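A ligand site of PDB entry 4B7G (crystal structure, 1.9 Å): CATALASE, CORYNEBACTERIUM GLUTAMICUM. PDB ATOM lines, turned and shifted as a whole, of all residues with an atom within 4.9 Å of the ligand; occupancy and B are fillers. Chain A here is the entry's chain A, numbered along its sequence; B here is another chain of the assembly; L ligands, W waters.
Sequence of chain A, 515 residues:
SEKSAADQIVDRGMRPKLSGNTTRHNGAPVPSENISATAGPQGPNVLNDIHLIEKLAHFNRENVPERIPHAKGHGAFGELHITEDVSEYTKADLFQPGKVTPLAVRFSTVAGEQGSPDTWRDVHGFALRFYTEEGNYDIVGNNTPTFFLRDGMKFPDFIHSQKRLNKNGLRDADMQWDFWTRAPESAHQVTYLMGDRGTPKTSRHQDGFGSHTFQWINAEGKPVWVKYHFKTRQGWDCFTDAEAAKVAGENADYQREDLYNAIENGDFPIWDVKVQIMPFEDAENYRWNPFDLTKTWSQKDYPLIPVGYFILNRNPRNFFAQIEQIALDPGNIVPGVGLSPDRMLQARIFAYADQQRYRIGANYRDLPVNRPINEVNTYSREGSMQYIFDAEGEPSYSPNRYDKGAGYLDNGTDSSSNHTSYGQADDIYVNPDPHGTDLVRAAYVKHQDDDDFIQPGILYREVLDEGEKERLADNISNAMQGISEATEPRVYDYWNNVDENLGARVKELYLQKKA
The guanidinium group (NH1) of Arg 106 is in salt-bridge range of an oxygen (O4) of the ligand, at 2.8 Å. The side-chain hydroxyl (OH) of Tyr 352 is bound to an iron atom (FE1) of the ligand, at 2.0 Å. The side-chain amide nitrogen (NE2) of Gln 355 is in hydrogen-bond range of an oxygen (O2) of the ligand (3.4 Å). The guanidinium group (NE) of Arg 67 lies within salt-bridge range of an oxygen (O3) of the ligand. The side-chain amide nitrogen (NE2) of Gln 356 lies within hydrogen-bond range of an oxygen (O1) of the ligand. An oxygen (O1) of the ligand is in salt-bridge range of the guanidinium group of Arg 359 (2.7 Å).
NH1 of Arg 348 sits at hydrogen-bond distance from NE2 of His 212. The backbone carbonyl oxygen (O) of Ser 108 is in hydrogen-bond range of the backbone NH (N) of Gly 125, at 2.8 Å. The guanidinium group (NH2) of Arg 67 lies within hydrogen-bond range of the backbone carbonyl oxygen (O) of Ile 326 (2.9 Å). The guanidinium group of Arg 359 sits at hydrogen-bond distance from the backbone carbonyl oxygen of Ile 326, 3.1 Å away. The backbone NH of Arg 106 is in hydrogen-bond range of the backbone carbonyl oxygen of Ala 127 (2.9 Å). NE2 of Gln 356 is in hydrogen-bond range of O of Leu 328 (2.9 Å). The backbone NH (N) of Phe 126 lies within hydrogen-bond range of the backbone carbonyl oxygen (O) of Gly 141 (2.9 Å). O of Ala 351 lies close to OD1 of Asn 60 of chain B, at 3.0 Å.
NE2 of His 70 lies close to N4 of the ligand, 3.4 Å away. Residues that only touch the ligand: Asn 142, Gly 141, Asn 60 of chain B, Met 344, Phe 155, Arg 348, Gly 125, Gly 210, Ser 211, Val 140, Gly 152, Ala 351, His 212, Leu 293, Phe 126, Pro 69, Leu 328, Ala 127, Ile 68 and Ala 347. Of the 33 residues printed, 27 come within 4 Å of the ligand. The nearest printed residue that does not touch the ligand is Phe 147 (4.03 Å).
Water W2 lies within hydrogen-bond range of an oxygen (O4) of the ligand (2.5 Å), the backbone carbonyl oxygen (O) of Arg 106 (2.7 Å) and the side-chain hydroxyl (OG) of Ser 108 (2.7 Å). Water W1 bridges ND2 of Asn 142 (2.9 Å) and OG of Ser 211 (2.9 Å).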
ATOM      1  N   ARG A  67      25.227  12.539  -8.044  1.00  0.00           N
ATOM      2  CA  ARG A  67      24.294  12.775  -6.930  1.00  0.00           C
ATOM      3  C   ARG A  67      24.415  11.697  -5.850  1.00  0.00           C
ATOM      4  O   ARG A  67      24.620  10.518  -6.165  1.00  0.00           O
ATOM      5  CB  ARG A  67      22.844  12.745  -7.429  1.00  0.00           C
ATOM      6  CG  ARG A  67      22.424  13.893  -8.326  1.00  0.00           C
ATOM      7  CD  ARG A  67      21.259  13.445  -9.221  1.00  0.00           C
ATOM      8  NE  ARG A  67      20.730  14.555 -10.025  1.00  0.00           N
ATOM      9  CZ  ARG A  67      21.291  14.985 -11.145  1.00  0.00           C
ATOM     10  NH1 ARG A  67      22.397  14.409 -11.604  1.00  0.00           N
ATOM     11  NH2 ARG A  67      20.750  16.004 -11.807  1.00  0.00           N
ATOM     12  N   ILE A  68      24.256  12.099  -4.592  1.00  0.00           N
ATOM     13  CA  ILE A  68      23.965  11.146  -3.525  1.00  0.00           C
ATOM     14  C   ILE A  68      22.714  11.582  -2.787  1.00  0.00           C
ATOM     15  O   ILE A  68      22.684  12.675  -2.229  1.00  0.00           O
ATOM     16  CB  ILE A  68      25.152  11.002  -2.527  1.00  0.00           C
ATOM     17  CG1 ILE A  68      24.716  10.209  -1.288  1.00  0.00           C
ATOM     18  CG2 ILE A  68      25.717  12.389  -2.140  1.00  0.00           C
ATOM     19  CD1 ILE A  68      25.911   9.702  -0.415  1.00  0.00           C
ATOM     20  N   PRO A  69      21.633  10.765  -2.820  1.00  0.00           N
ATOM     21  CA  PRO A  69      21.492   9.555  -3.639  1.00  0.00           C
ATOM     22  C   PRO A  69      20.955   9.912  -5.030  1.00  0.00           C
ATOM     23  O   PRO A  69      21.033  11.093  -5.407  1.00  0.00           O
ATOM     24  CB  PRO A  69      20.453   8.723  -2.860  1.00  0.00           C
ATOM     25  CG  PRO A  69      19.769   9.712  -1.865  1.00  0.00           C
ATOM     26  CD  PRO A  69      20.390  11.086  -2.095  1.00  0.00           C
ATOM     27  N   HIS A  70      20.437   8.920  -5.749  1.00  0.00           N
ATOM     28  CA  HIS A  70      19.789   9.096  -7.059  1.00  0.00           C
ATOM     29  C   HIS A  70      20.782   9.393  -8.187  1.00  0.00           C
ATOM     30  O   HIS A  70      20.445  10.058  -9.156  1.00  0.00           O
ATOM     31  CB  HIS A  70      18.703  10.181  -7.019  1.00  0.00           C
ATOM     32  CG  HIS A  70      17.557   9.877  -6.086  1.00  0.00           C
ATOM     33  ND1 HIS A  70      16.338   9.427  -6.543  1.00  0.00           N
ATOM     34  CD2 HIS A  70      17.432  10.011  -4.745  1.00  0.00           C
ATOM     35  CE1 HIS A  70      15.511   9.284  -5.515  1.00  0.00           C
ATOM     36  NE2 HIS A  70      16.152   9.634  -4.411  1.00  0.00           N
ATOM     37  N   ARG A 106      13.289  14.394 -14.305  1.00  0.00           N
ATOM     38  CA  ARG A 106      14.346  13.390 -14.201  1.00  0.00           C
ATOM     39  C   ARG A 106      13.835  12.209 -13.394  1.00  0.00           C
ATOM     40  O   ARG A 106      13.275  12.391 -12.297  1.00  0.00           O
ATOM     41  CB  ARG A 106      15.604  13.962 -13.529  1.00  0.00           C
ATOM     42  CG  ARG A 106      16.817  13.004 -13.595  1.00  0.00           C
ATOM     43  CD  ARG A 106      18.059  13.690 -13.072  1.00  0.00           C
ATOM     44  NE  ARG A 106      19.233  12.821 -13.034  1.00  0.00           N
ATOM     45  CZ  ARG A 106      19.543  12.019 -12.019  1.00  0.00           C
ATOM     46  NH1 ARG A 106      18.764  11.937 -10.941  1.00  0.00           N
ATOM     47  NH2 ARG A 106      20.641  11.272 -12.089  1.00  0.00           N
ATOM     48  N   SER A 108      14.936   8.225 -11.853  1.00  0.00           N
ATOM     49  CA  SER A 108      16.165   7.667 -11.301  1.00  0.00           C
ATOM     50  C   SER A 108      15.885   6.496 -10.393  1.00  0.00           C
ATOM     51  O   SER A 108      14.734   6.250 -10.019  1.00  0.00           O
ATOM     52  CB  SER A 108      16.885   8.733 -10.472  1.00  0.00           C
ATOM     53  OG  SER A 108      16.016   9.224  -9.456  1.00  0.00           O
ATOM     54  N   GLY A 125      12.975   7.748  -8.408  1.00  0.00           N
ATOM     55  CA  GLY A 125      12.743   9.179  -8.347  1.00  0.00           C
ATOM     56  C   GLY A 125      11.851   9.662  -9.478  1.00  0.00           C
ATOM     57  O   GLY A 125      11.906   9.119 -10.588  1.00  0.00           O
ATOM     58  N   PHE A 126      11.055  10.688  -9.205  1.00  0.00           N
ATOM     59  CA  PHE A 126      10.088  11.224 -10.162  1.00  0.00           C
ATOM     60  C   PHE A 126      10.114  12.745  -9.927  1.00  0.00           C
ATOM     61  O   PHE A 126       9.267  13.297  -9.205  1.00  0.00           O
ATOM     62  CB  PHE A 126       8.701  10.633  -9.862  1.00  0.00           C
ATOM     63  CG  PHE A 126       7.711  10.713 -11.016  1.00  0.00           C
ATOM     64  CD1 PHE A 126       7.217  11.935 -11.459  1.00  0.00           C
ATOM     65  CD2 PHE A 126       7.223   9.548 -11.598  1.00  0.00           C
ATOM     66  CE1 PHE A 126       6.299  11.999 -12.494  1.00  0.00           C
ATOM     67  CE2 PHE A 126       6.288   9.596 -12.637  1.00  0.00           C
ATOM     68  CZ  PHE A 126       5.822  10.822 -13.094  1.00  0.00           C
ATOM     69  N   ALA A 127      11.099  13.422 -10.517  1.00  0.00           N
ATOM     70  CA  ALA A 127      11.389  14.802 -10.154  1.00  0.00           C
ATOM     71  C   ALA A 127      11.079  15.783 -11.286  1.00  0.00           C
ATOM     72  O   ALA A 127      11.711  15.752 -12.337  1.00  0.00           O
ATOM     73  CB  ALA A 127      12.857  14.940  -9.732  1.00  0.00           C
ATOM     74  N   VAL A 140       9.799  17.562  -6.497  1.00  0.00           N
ATOM     75  CA  VAL A 140      10.779  16.476  -6.530  1.00  0.00           C
ATOM     76  C   VAL A 140      10.164  15.303  -5.784  1.00  0.00           C
ATOM     77  O   VAL A 140      10.276  15.199  -4.557  1.00  0.00           O
ATOM     78  CB  VAL A 140      12.110  16.931  -5.892  1.00  0.00           C
ATOM     79  CG1 VAL A 140      13.185  15.829  -6.006  1.00  0.00           C
ATOM     80  CG2 VAL A 140      12.585  18.248  -6.558  1.00  0.00           C
ATOM     81  N   GLY A 141       9.514  14.421  -6.531  1.00  0.00           N
ATOM     82  CA  GLY A 141       8.788  13.329  -5.913  1.00  0.00           C
ATOM     83  C   GLY A 141       9.410  11.976  -6.154  1.00  0.00           C
ATOM     84  O   GLY A 141      10.550  11.889  -6.631  1.00  0.00           O
ATOM     85  N   ASN A 142       8.686  10.924  -5.790  1.00  0.00           N
ATOM     86  CA  ASN A 142       9.128   9.544  -6.003  1.00  0.00           C
ATOM     87  C   ASN A 142       7.944   8.777  -6.550  1.00  0.00           C
ATOM     88  O   ASN A 142       6.834   9.314  -6.626  1.00  0.00           O
ATOM     89  CB  ASN A 142       9.574   8.899  -4.673  1.00  0.00           C
ATOM     90  CG  ASN A 142      11.044   9.164  -4.341  1.00  0.00           C
ATOM     91  OD1 ASN A 142      11.902   9.255  -5.222  1.00  0.00           O
ATOM     92  ND2 ASN A 142      11.337   9.257  -3.038  1.00  0.00           N
ATOM     93  N   PHE A 147       7.329   7.196   2.359  1.00  0.00           N
ATOM     94  CA  PHE A 147       8.784   6.971   2.386  1.00  0.00           C
ATOM     95  C   PHE A 147       9.216   6.275   3.675  1.00  0.00           C
ATOM     96  O   PHE A 147       8.395   6.060   4.572  1.00  0.00           O
ATOM     97  CB  PHE A 147       9.531   8.292   2.213  1.00  0.00           C
ATOM     98  CG  PHE A 147      10.954   8.143   1.696  1.00  0.00           C
ATOM     99  CD1 PHE A 147      11.199   7.672   0.413  1.00  0.00           C
ATOM    100  CD2 PHE A 147      12.024   8.525   2.486  1.00  0.00           C
ATOM    101  CE1 PHE A 147      12.514   7.562  -0.082  1.00  0.00           C
ATOM    102  CE2 PHE A 147      13.343   8.408   2.021  1.00  0.00           C
ATOM    103  CZ  PHE A 147      13.580   7.925   0.730  1.00  0.00           C
ATOM    104  N   GLY A 152      14.559  13.861   9.058  1.00  0.00           N
ATOM    105  CA  GLY A 152      15.726  14.028   8.202  1.00  0.00           C
ATOM    106  C   GLY A 152      17.018  13.638   8.883  1.00  0.00           C
ATOM    107  O   GLY A 152      18.000  13.270   8.224  1.00  0.00           O
ATOM    108  N   PHE A 155      18.161  10.340   7.628  1.00  0.00           N
ATOM    109  CA  PHE A 155      18.324  10.103   6.194  1.00  0.00           C
ATOM    110  C   PHE A 155      19.712   9.571   5.793  1.00  0.00           C
ATOM    111  O   PHE A 155      19.785   8.584   5.046  1.00  0.00           O
ATOM    112  CB  PHE A 155      17.918  11.335   5.375  1.00  0.00           C
ATOM    113  CG  PHE A 155      17.930  11.116   3.892  1.00  0.00           C
ATOM    114  CD1 PHE A 155      16.940  10.337   3.274  1.00  0.00           C
ATOM    115  CD2 PHE A 155      18.926  11.677   3.098  1.00  0.00           C
ATOM    116  CE1 PHE A 155      16.943  10.130   1.896  1.00  0.00           C
ATOM    117  CE2 PHE A 155      18.937  11.473   1.717  1.00  0.00           C
ATOM    118  CZ  PHE A 155      17.948  10.711   1.122  1.00  0.00           C
ATOM    119  N   PHE A 209       4.496  10.757  -7.213  1.00  0.00           N
ATOM    120  CA  PHE A 209       3.840  11.374  -6.053  1.00  0.00           C
ATOM    121  C   PHE A 209       4.719  12.459  -5.454  1.00  0.00           C
ATOM    122  O   PHE A 209       5.948  12.359  -5.485  1.00  0.00           O
ATOM    123  CB  PHE A 209       3.607  10.328  -4.967  1.00  0.00           C
ATOM    124  CG  PHE A 209       2.819   9.139  -5.430  1.00  0.00           C
ATOM    125  CD1 PHE A 209       3.461   8.047  -6.003  1.00  0.00           C
ATOM    126  CD2 PHE A 209       1.428   9.087  -5.258  1.00  0.00           C
ATOM    127  CE1 PHE A 209       2.746   6.934  -6.427  1.00  0.00           C
ATOM    128  CE2 PHE A 209       0.697   7.979  -5.685  1.00  0.00           C
ATOM    129  CZ  PHE A 209       1.351   6.896  -6.274  1.00  0.00           C
ATOM    130  N   GLY A 210       4.090  13.494  -4.893  1.00  0.00           N
ATOM    131  CA  GLY A 210       4.843  14.477  -4.120  1.00  0.00           C
ATOM    132  C   GLY A 210       5.266  13.855  -2.787  1.00  0.00           C
ATOM    133  O   GLY A 210       6.243  14.294  -2.171  1.00  0.00           O
ATOM    134  N   SER A 211       4.535  12.815  -2.397  1.00  0.00           N
ATOM    135  CA  SER A 211       4.684  12.125  -1.106  1.00  0.00           C
ATOM    136  C   SER A 211       4.338  13.000   0.106  1.00  0.00           C
ATOM    137  O   SER A 211       3.399  12.679   0.850  1.00  0.00           O
ATOM    138  CB  SER A 211       6.066  11.464  -0.949  1.00  0.00           C
ATOM    139  OG  SER A 211       6.360  10.630  -2.065  1.00  0.00           O
ATOM    140  N   HIS A 212       5.074  14.082   0.317  1.00  0.00           N
ATOM    141  CA  HIS A 212       4.800  14.992   1.431  1.00  0.00           C
ATOM    142  C   HIS A 212       3.445  15.685   1.320  1.00  0.00           C
ATOM    143  O   HIS A 212       2.933  15.922   0.229  1.00  0.00           O
ATOM    144  CB  HIS A 212       5.837  16.121   1.525  1.00  0.00           C
ATOM    145  CG  HIS A 212       7.258  15.653   1.648  1.00  0.00           C
ATOM    146  ND1 HIS A 212       7.777  15.120   2.808  1.00  0.00           N
ATOM    147  CD2 HIS A 212       8.281  15.703   0.761  1.00  0.00           C
ATOM    148  CE1 HIS A 212       9.053  14.836   2.628  1.00  0.00           C
ATOM    149  NE2 HIS A 212       9.383  15.171   1.387  1.00  0.00           N
ATOM    150  N   LEU A 293       5.330  11.629   7.006  1.00  0.00           N
ATOM    151  CA  LEU A 293       5.579  11.114   5.650  1.00  0.00           C
ATOM    152  C   LEU A 293       5.279   9.633   5.506  1.00  0.00           C
ATOM    153  O   LEU A 293       4.889   9.169   4.417  1.00  0.00           O
ATOM    154  CB  LEU A 293       7.025  11.400   5.250  1.00  0.00           C
ATOM    155  CG  LEU A 293       7.494  10.987   3.853  1.00  0.00           C
ATOM    156  CD1 LEU A 293       6.607  11.583   2.763  1.00  0.00           C
ATOM    157  CD2 LEU A 293       8.960  11.410   3.667  1.00  0.00           C
ATOM    158  N   ILE A 326      21.143  19.215 -14.278  1.00  0.00           N
ATOM    159  CA  ILE A 326      19.926  19.806 -13.720  1.00  0.00           C
ATOM    160  C   ILE A 326      20.008  19.771 -12.193  1.00  0.00           C
ATOM    161  O   ILE A 326      20.604  18.854 -11.615  1.00  0.00           O
ATOM    162  CB  ILE A 326      18.613  19.167 -14.238  1.00  0.00           C
ATOM    163  CG1 ILE A 326      17.437  20.131 -14.022  1.00  0.00           C
ATOM    164  CG2 ILE A 326      18.313  17.829 -13.557  1.00  0.00           C
ATOM    165  CD1 ILE A 326      16.203  19.820 -14.905  1.00  0.00           C
ATOM    166  N   ALA A 327      19.459  20.792 -11.550  1.00  0.00           N
ATOM    167  CA  ALA A 327      19.511  20.889 -10.097  1.00  0.00           C
ATOM    168  C   ALA A 327      18.075  20.978  -9.546  1.00  0.00           C
ATOM    169  O   ALA A 327      17.567  22.063  -9.261  1.00  0.00           O
ATOM    170  CB  ALA A 327      20.316  22.121  -9.683  1.00  0.00           C
ATOM    171  N   LEU A 328      17.431  19.814  -9.419  1.00  0.00           N
ATOM    172  CA  LEU A 328      16.043  19.765  -8.981  1.00  0.00           C
ATOM    173  C   LEU A 328      16.001  19.892  -7.458  1.00  0.00           C
ATOM    174  O   LEU A 328      16.823  19.281  -6.761  1.00  0.00           O
ATOM    175  CB  LEU A 328      15.369  18.482  -9.496  1.00  0.00           C
ATOM    176  CG  LEU A 328      15.329  18.471 -11.035  1.00  0.00           C
ATOM    177  CD1 LEU A 328      15.146  17.053 -11.620  1.00  0.00           C
ATOM    178  CD2 LEU A 328      14.205  19.386 -11.549  1.00  0.00           C
ATOM    179  N   MET A 344      10.887  15.640   7.372  1.00  0.00           N
ATOM    180  CA  MET A 344      11.696  15.154   6.251  1.00  0.00           C
ATOM    181  C   MET A 344      11.727  16.241   5.199  1.00  0.00           C
ATOM    182  O   MET A 344      12.795  16.570   4.650  1.00  0.00           O
ATOM    183  CB  MET A 344      11.113  13.872   5.670  1.00  0.00           C
ATOM    184  CG  MET A 344      11.239  12.686   6.628  1.00  0.00           C
ATOM    185  SD  MET A 344      12.853  11.887   6.506  1.00  0.00           S
ATOM    186  CE  MET A 344      12.635  11.023   4.953  1.00  0.00           C
ATOM    187  N   ALA A 347      13.937  19.294   6.238  1.00  0.00           N
ATOM    188  CA  ALA A 347      15.346  18.985   6.024  1.00  0.00           C
ATOM    189  C   ALA A 347      15.724  19.053   4.536  1.00  0.00           C
ATOM    190  O   ALA A 347      16.792  19.570   4.193  1.00  0.00           O
ATOM    191  CB  ALA A 347      15.695  17.612   6.591  1.00  0.00           C
ATOM    192  N   ARG A 348      14.870  18.502   3.672  1.00  0.00           N
ATOM    193  CA  ARG A 348      15.117  18.542   2.212  1.00  0.00           C
ATOM    194  C   ARG A 348      15.237  19.974   1.682  1.00  0.00           C
ATOM    195  O   ARG A 348      16.043  20.254   0.775  1.00  0.00           O
ATOM    196  CB  ARG A 348      13.998  17.818   1.448  1.00  0.00           C
ATOM    197  CG  ARG A 348      13.854  16.325   1.762  1.00  0.00           C
ATOM    198  CD  ARG A 348      12.689  15.705   0.963  1.00  0.00           C
ATOM    199  NE  ARG A 348      12.998  15.651  -0.469  1.00  0.00           N
ATOM    200  CZ  ARG A 348      12.084  15.742  -1.436  1.00  0.00           C
ATOM    201  NH1 ARG A 348      10.803  15.895  -1.120  1.00  0.00           N
ATOM    202  NH2 ARG A 348      12.447  15.696  -2.704  1.00  0.00           N
ATOM    203  N   ALA A 351      18.739  20.653   2.089  1.00  0.00           N
ATOM    204  CA  ALA A 351      19.788  19.737   1.638  1.00  0.00           C
ATOM    205  C   ALA A 351      20.139  19.754   0.136  1.00  0.00           C
ATOM    206  O   ALA A 351      21.279  19.480  -0.235  1.00  0.00           O
ATOM    207  CB  ALA A 351      19.462  18.309   2.089  1.00  0.00           C
ATOM    208  N   TYR A 352      19.173  20.041  -0.733  1.00  0.00           N
ATOM    209  CA  TYR A 352      19.429  19.878  -2.172  1.00  0.00           C
ATOM    210  C   TYR A 352      20.330  20.978  -2.683  1.00  0.00           C
ATOM    211  O   TYR A 352      21.327  20.700  -3.364  1.00  0.00           O
ATOM    212  CB  TYR A 352      18.119  19.860  -2.981  1.00  0.00           C
ATOM    213  CG  TYR A 352      17.318  18.598  -2.776  1.00  0.00           C
ATOM    214  CD1 TYR A 352      16.838  18.263  -1.519  1.00  0.00           C
ATOM    215  CD2 TYR A 352      17.040  17.746  -3.832  1.00  0.00           C
ATOM    216  CE1 TYR A 352      16.102  17.106  -1.315  1.00  0.00           C
ATOM    217  CE2 TYR A 352      16.304  16.581  -3.639  1.00  0.00           C
ATOM    218  CZ  TYR A 352      15.837  16.272  -2.375  1.00  0.00           C
ATOM    219  OH  TYR A 352      15.105  15.120  -2.183  1.00  0.00           O
ATOM    220  N   GLN A 355      23.837  20.457  -1.562  1.00  0.00           N
ATOM    221  CA  GLN A 355      24.655  19.515  -2.328  1.00  0.00           C
ATOM    222  C   GLN A 355      24.993  20.076  -3.719  1.00  0.00           C
ATOM    223  O   GLN A 355      26.107  19.875  -4.227  1.00  0.00           O
ATOM    224  CB  GLN A 355      23.971  18.142  -2.468  1.00  0.00           C
ATOM    225  CG  GLN A 355      24.852  17.175  -3.288  1.00  0.00           C
ATOM    226  CD  GLN A 355      24.407  15.718  -3.261  1.00  0.00           C
ATOM    227  OE1 GLN A 355      23.750  15.255  -2.320  1.00  0.00           O
ATOM    228  NE2 GLN A 355      24.784  14.988  -4.308  1.00  0.00           N
ATOM    229  N   GLN A 356      24.030  20.787  -4.306  1.00  0.00           N
ATOM    230  CA  GLN A 356      24.200  21.326  -5.664  1.00  0.00           C
ATOM    231  C   GLN A 356      25.311  22.364  -5.736  1.00  0.00           C
ATOM    232  O   GLN A 356      26.055  22.442  -6.731  1.00  0.00           O
ATOM    233  CB  GLN A 356      22.848  21.854  -6.170  1.00  0.00           C
ATOM    234  CG  GLN A 356      21.909  20.695  -6.524  1.00  0.00           C
ATOM    235  CD  GLN A 356      20.441  21.026  -6.392  1.00  0.00           C
ATOM    236  OE1 GLN A 356      20.051  22.163  -6.081  1.00  0.00           O
ATOM    237  NE2 GLN A 356      19.593  20.011  -6.610  1.00  0.00           N
ATOM    238  N   ARG A 359      28.230  19.910  -5.819  1.00  0.00           N
ATOM    239  CA  ARG A 359      28.209  18.952  -6.918  1.00  0.00           C
ATOM    240  C   ARG A 359      28.405  19.632  -8.264  1.00  0.00           C
ATOM    241  O   ARG A 359      29.101  19.112  -9.156  1.00  0.00           O
ATOM    242  CB  ARG A 359      26.870  18.204  -6.900  1.00  0.00           C
ATOM    243  CG  ARG A 359      26.617  17.348  -8.101  1.00  0.00           C
ATOM    244  CD  ARG A 359      25.416  16.419  -7.876  1.00  0.00           C
ATOM    245  NE  ARG A 359      24.113  17.079  -7.993  1.00  0.00           N
ATOM    246  CZ  ARG A 359      23.563  17.451  -9.143  1.00  0.00           C
ATOM    247  NH1 ARG A 359      24.219  17.255 -10.287  1.00  0.00           N
ATOM    248  NH2 ARG A 359      22.358  18.025  -9.170  1.00  0.00           N
ATOM    249  N   LEU B  56      23.968  16.276   7.535  1.00  0.00           N
ATOM    250  CA  LEU B  56      23.440  16.393   6.174  1.00  0.00           C
ATOM    251  C   LEU B  56      24.497  16.944   5.227  1.00  0.00           C
ATOM    252  O   LEU B  56      24.676  16.441   4.117  1.00  0.00           O
ATOM    253  CB  LEU B  56      22.180  17.270   6.144  1.00  0.00           C
ATOM    254  CG  LEU B  56      20.926  16.675   6.803  1.00  0.00           C
ATOM    255  CD1 LEU B  56      19.764  17.653   6.758  1.00  0.00           C
ATOM    256  CD2 LEU B  56      20.536  15.345   6.159  1.00  0.00           C
ATOM    257  N   ASN B  60      26.134  15.248   1.988  1.00  0.00           N
ATOM    258  CA  ASN B  60      26.023  15.892   0.675  1.00  0.00           C
ATOM    259  C   ASN B  60      27.341  15.963  -0.095  1.00  0.00           C
ATOM    260  O   ASN B  60      27.347  16.184  -1.324  1.00  0.00           O
ATOM    261  CB  ASN B  60      25.504  17.324   0.829  1.00  0.00           C
ATOM    262  CG  ASN B  60      24.015  17.374   1.013  1.00  0.00           C
ATOM    263  OD1 ASN B  60      23.470  18.348   1.551  1.00  0.00           O
ATOM    264  ND2 ASN B  60      23.335  16.323   0.578  1.00  0.00           N
HETATM  265  C1  LIG L   1      18.021  13.460  -4.608  1.00  0.00           C
HETATM  266  C2  LIG L   1      18.328  14.685   0.105  1.00  0.00           C
HETATM  267  C3  LIG L   1      14.149  12.344   0.930  1.00  0.00           C
HETATM  268  C4  LIG L   1      13.284  12.443  -3.853  1.00  0.00           C
HETATM  269  C5  LIG L   1      18.463  14.019  -3.423  1.00  0.00           C
HETATM  270  C6  LIG L   1      19.639  14.852  -3.234  1.00  0.00           C
HETATM  271  C7  LIG L   1      19.700  15.189  -1.942  1.00  0.00           C
HETATM  272  C8  LIG L   1      18.589  14.578  -1.253  1.00  0.00           C
HETATM  273  C9  LIG L   1      20.769  16.073  -1.263  1.00  0.00           C
HETATM  274  C10 LIG L   1      20.638  15.277  -4.331  1.00  0.00           C
HETATM  275  C11 LIG L   1      20.077  16.425  -5.161  1.00  0.00           C
HETATM  276  C12 LIG L   1      21.116  16.959  -6.112  1.00  0.00           C
HETATM  277  O1  LIG L   1      20.703  17.525  -7.154  1.00  0.00           O
HETATM  278  O2  LIG L   1      22.342  16.847  -5.830  1.00  0.00           O
HETATM  279  C13 LIG L   1      17.234  14.131   0.735  1.00  0.00           C
HETATM  280  C14 LIG L   1      16.938  14.217   2.153  1.00  0.00           C
HETATM  281  C15 LIG L   1      15.795  13.545   2.385  1.00  0.00           C
HETATM  282  C16 LIG L   1      15.313  13.062   1.115  1.00  0.00           C
HETATM  283  C17 LIG L   1      17.875  14.930   3.159  1.00  0.00           C
HETATM  284  C18 LIG L   1      15.028  13.343   3.703  1.00  0.00           C
HETATM  285  C19 LIG L   1      15.093  14.233   4.708  1.00  0.00           C
HETATM  286  C20 LIG L   1      13.477  12.326  -0.285  1.00  0.00           C
HETATM  287  C21 LIG L   1      12.048  12.199  -0.490  1.00  0.00           C
HETATM  288  C22 LIG L   1      11.828  12.212  -1.829  1.00  0.00           C
HETATM  289  C23 LIG L   1      13.103  12.380  -2.492  1.00  0.00           C
HETATM  290  C24 LIG L   1      11.003  12.033   0.652  1.00  0.00           C
HETATM  291  C25 LIG L   1      10.488  12.148  -2.595  1.00  0.00           C
HETATM  292  C26 LIG L   1       9.329  12.568  -2.058  1.00  0.00           C
HETATM  293  C27 LIG L   1      14.475  12.662  -4.504  1.00  0.00           C
HETATM  294  C28 LIG L   1      14.658  12.599  -5.932  1.00  0.00           C
HETATM  295  C29 LIG L   1      16.126  12.913  -6.163  1.00  0.00           C
HETATM  296  C30 LIG L   1      16.698  13.144  -4.859  1.00  0.00           C
HETATM  297  C31 LIG L   1      13.598  12.282  -7.011  1.00  0.00           C
HETATM  298  C32 LIG L   1      16.818  12.987  -7.534  1.00  0.00           C
HETATM  299  C33 LIG L   1      16.404  14.318  -8.162  1.00  0.00           C
HETATM  300  C34 LIG L   1      16.965  14.286  -9.546  1.00  0.00           C
HETATM  301  O3  LIG L   1      17.910  15.073  -9.839  1.00  0.00           O
HETATM  302  O4  LIG L   1      16.458  13.442 -10.336  1.00  0.00           O
HETATM  303  N1  LIG L   1      17.846  13.879  -2.184  1.00  0.00           N
HETATM  304  N2  LIG L   1      16.226  13.419   0.131  1.00  0.00           N
HETATM  305  N3  LIG L   1      14.093  12.444  -1.526  1.00  0.00           N
HETATM  306  N4  LIG L   1      15.692  12.972  -3.914  1.00  0.00           N
HETATM  307 FE1  LIG L   1      15.869  13.332  -1.875  1.00  0.00          FE
HETATM  308  O   HOH W   1       8.951   9.424  -1.357  1.00  0.00           O
HETATM  309  O   HOH W   2      14.777  11.538 -10.212  1.00  0.00           O
HETATM  310  O   HOH W   3      19.011  17.285  -9.179  1.00  0.00           O
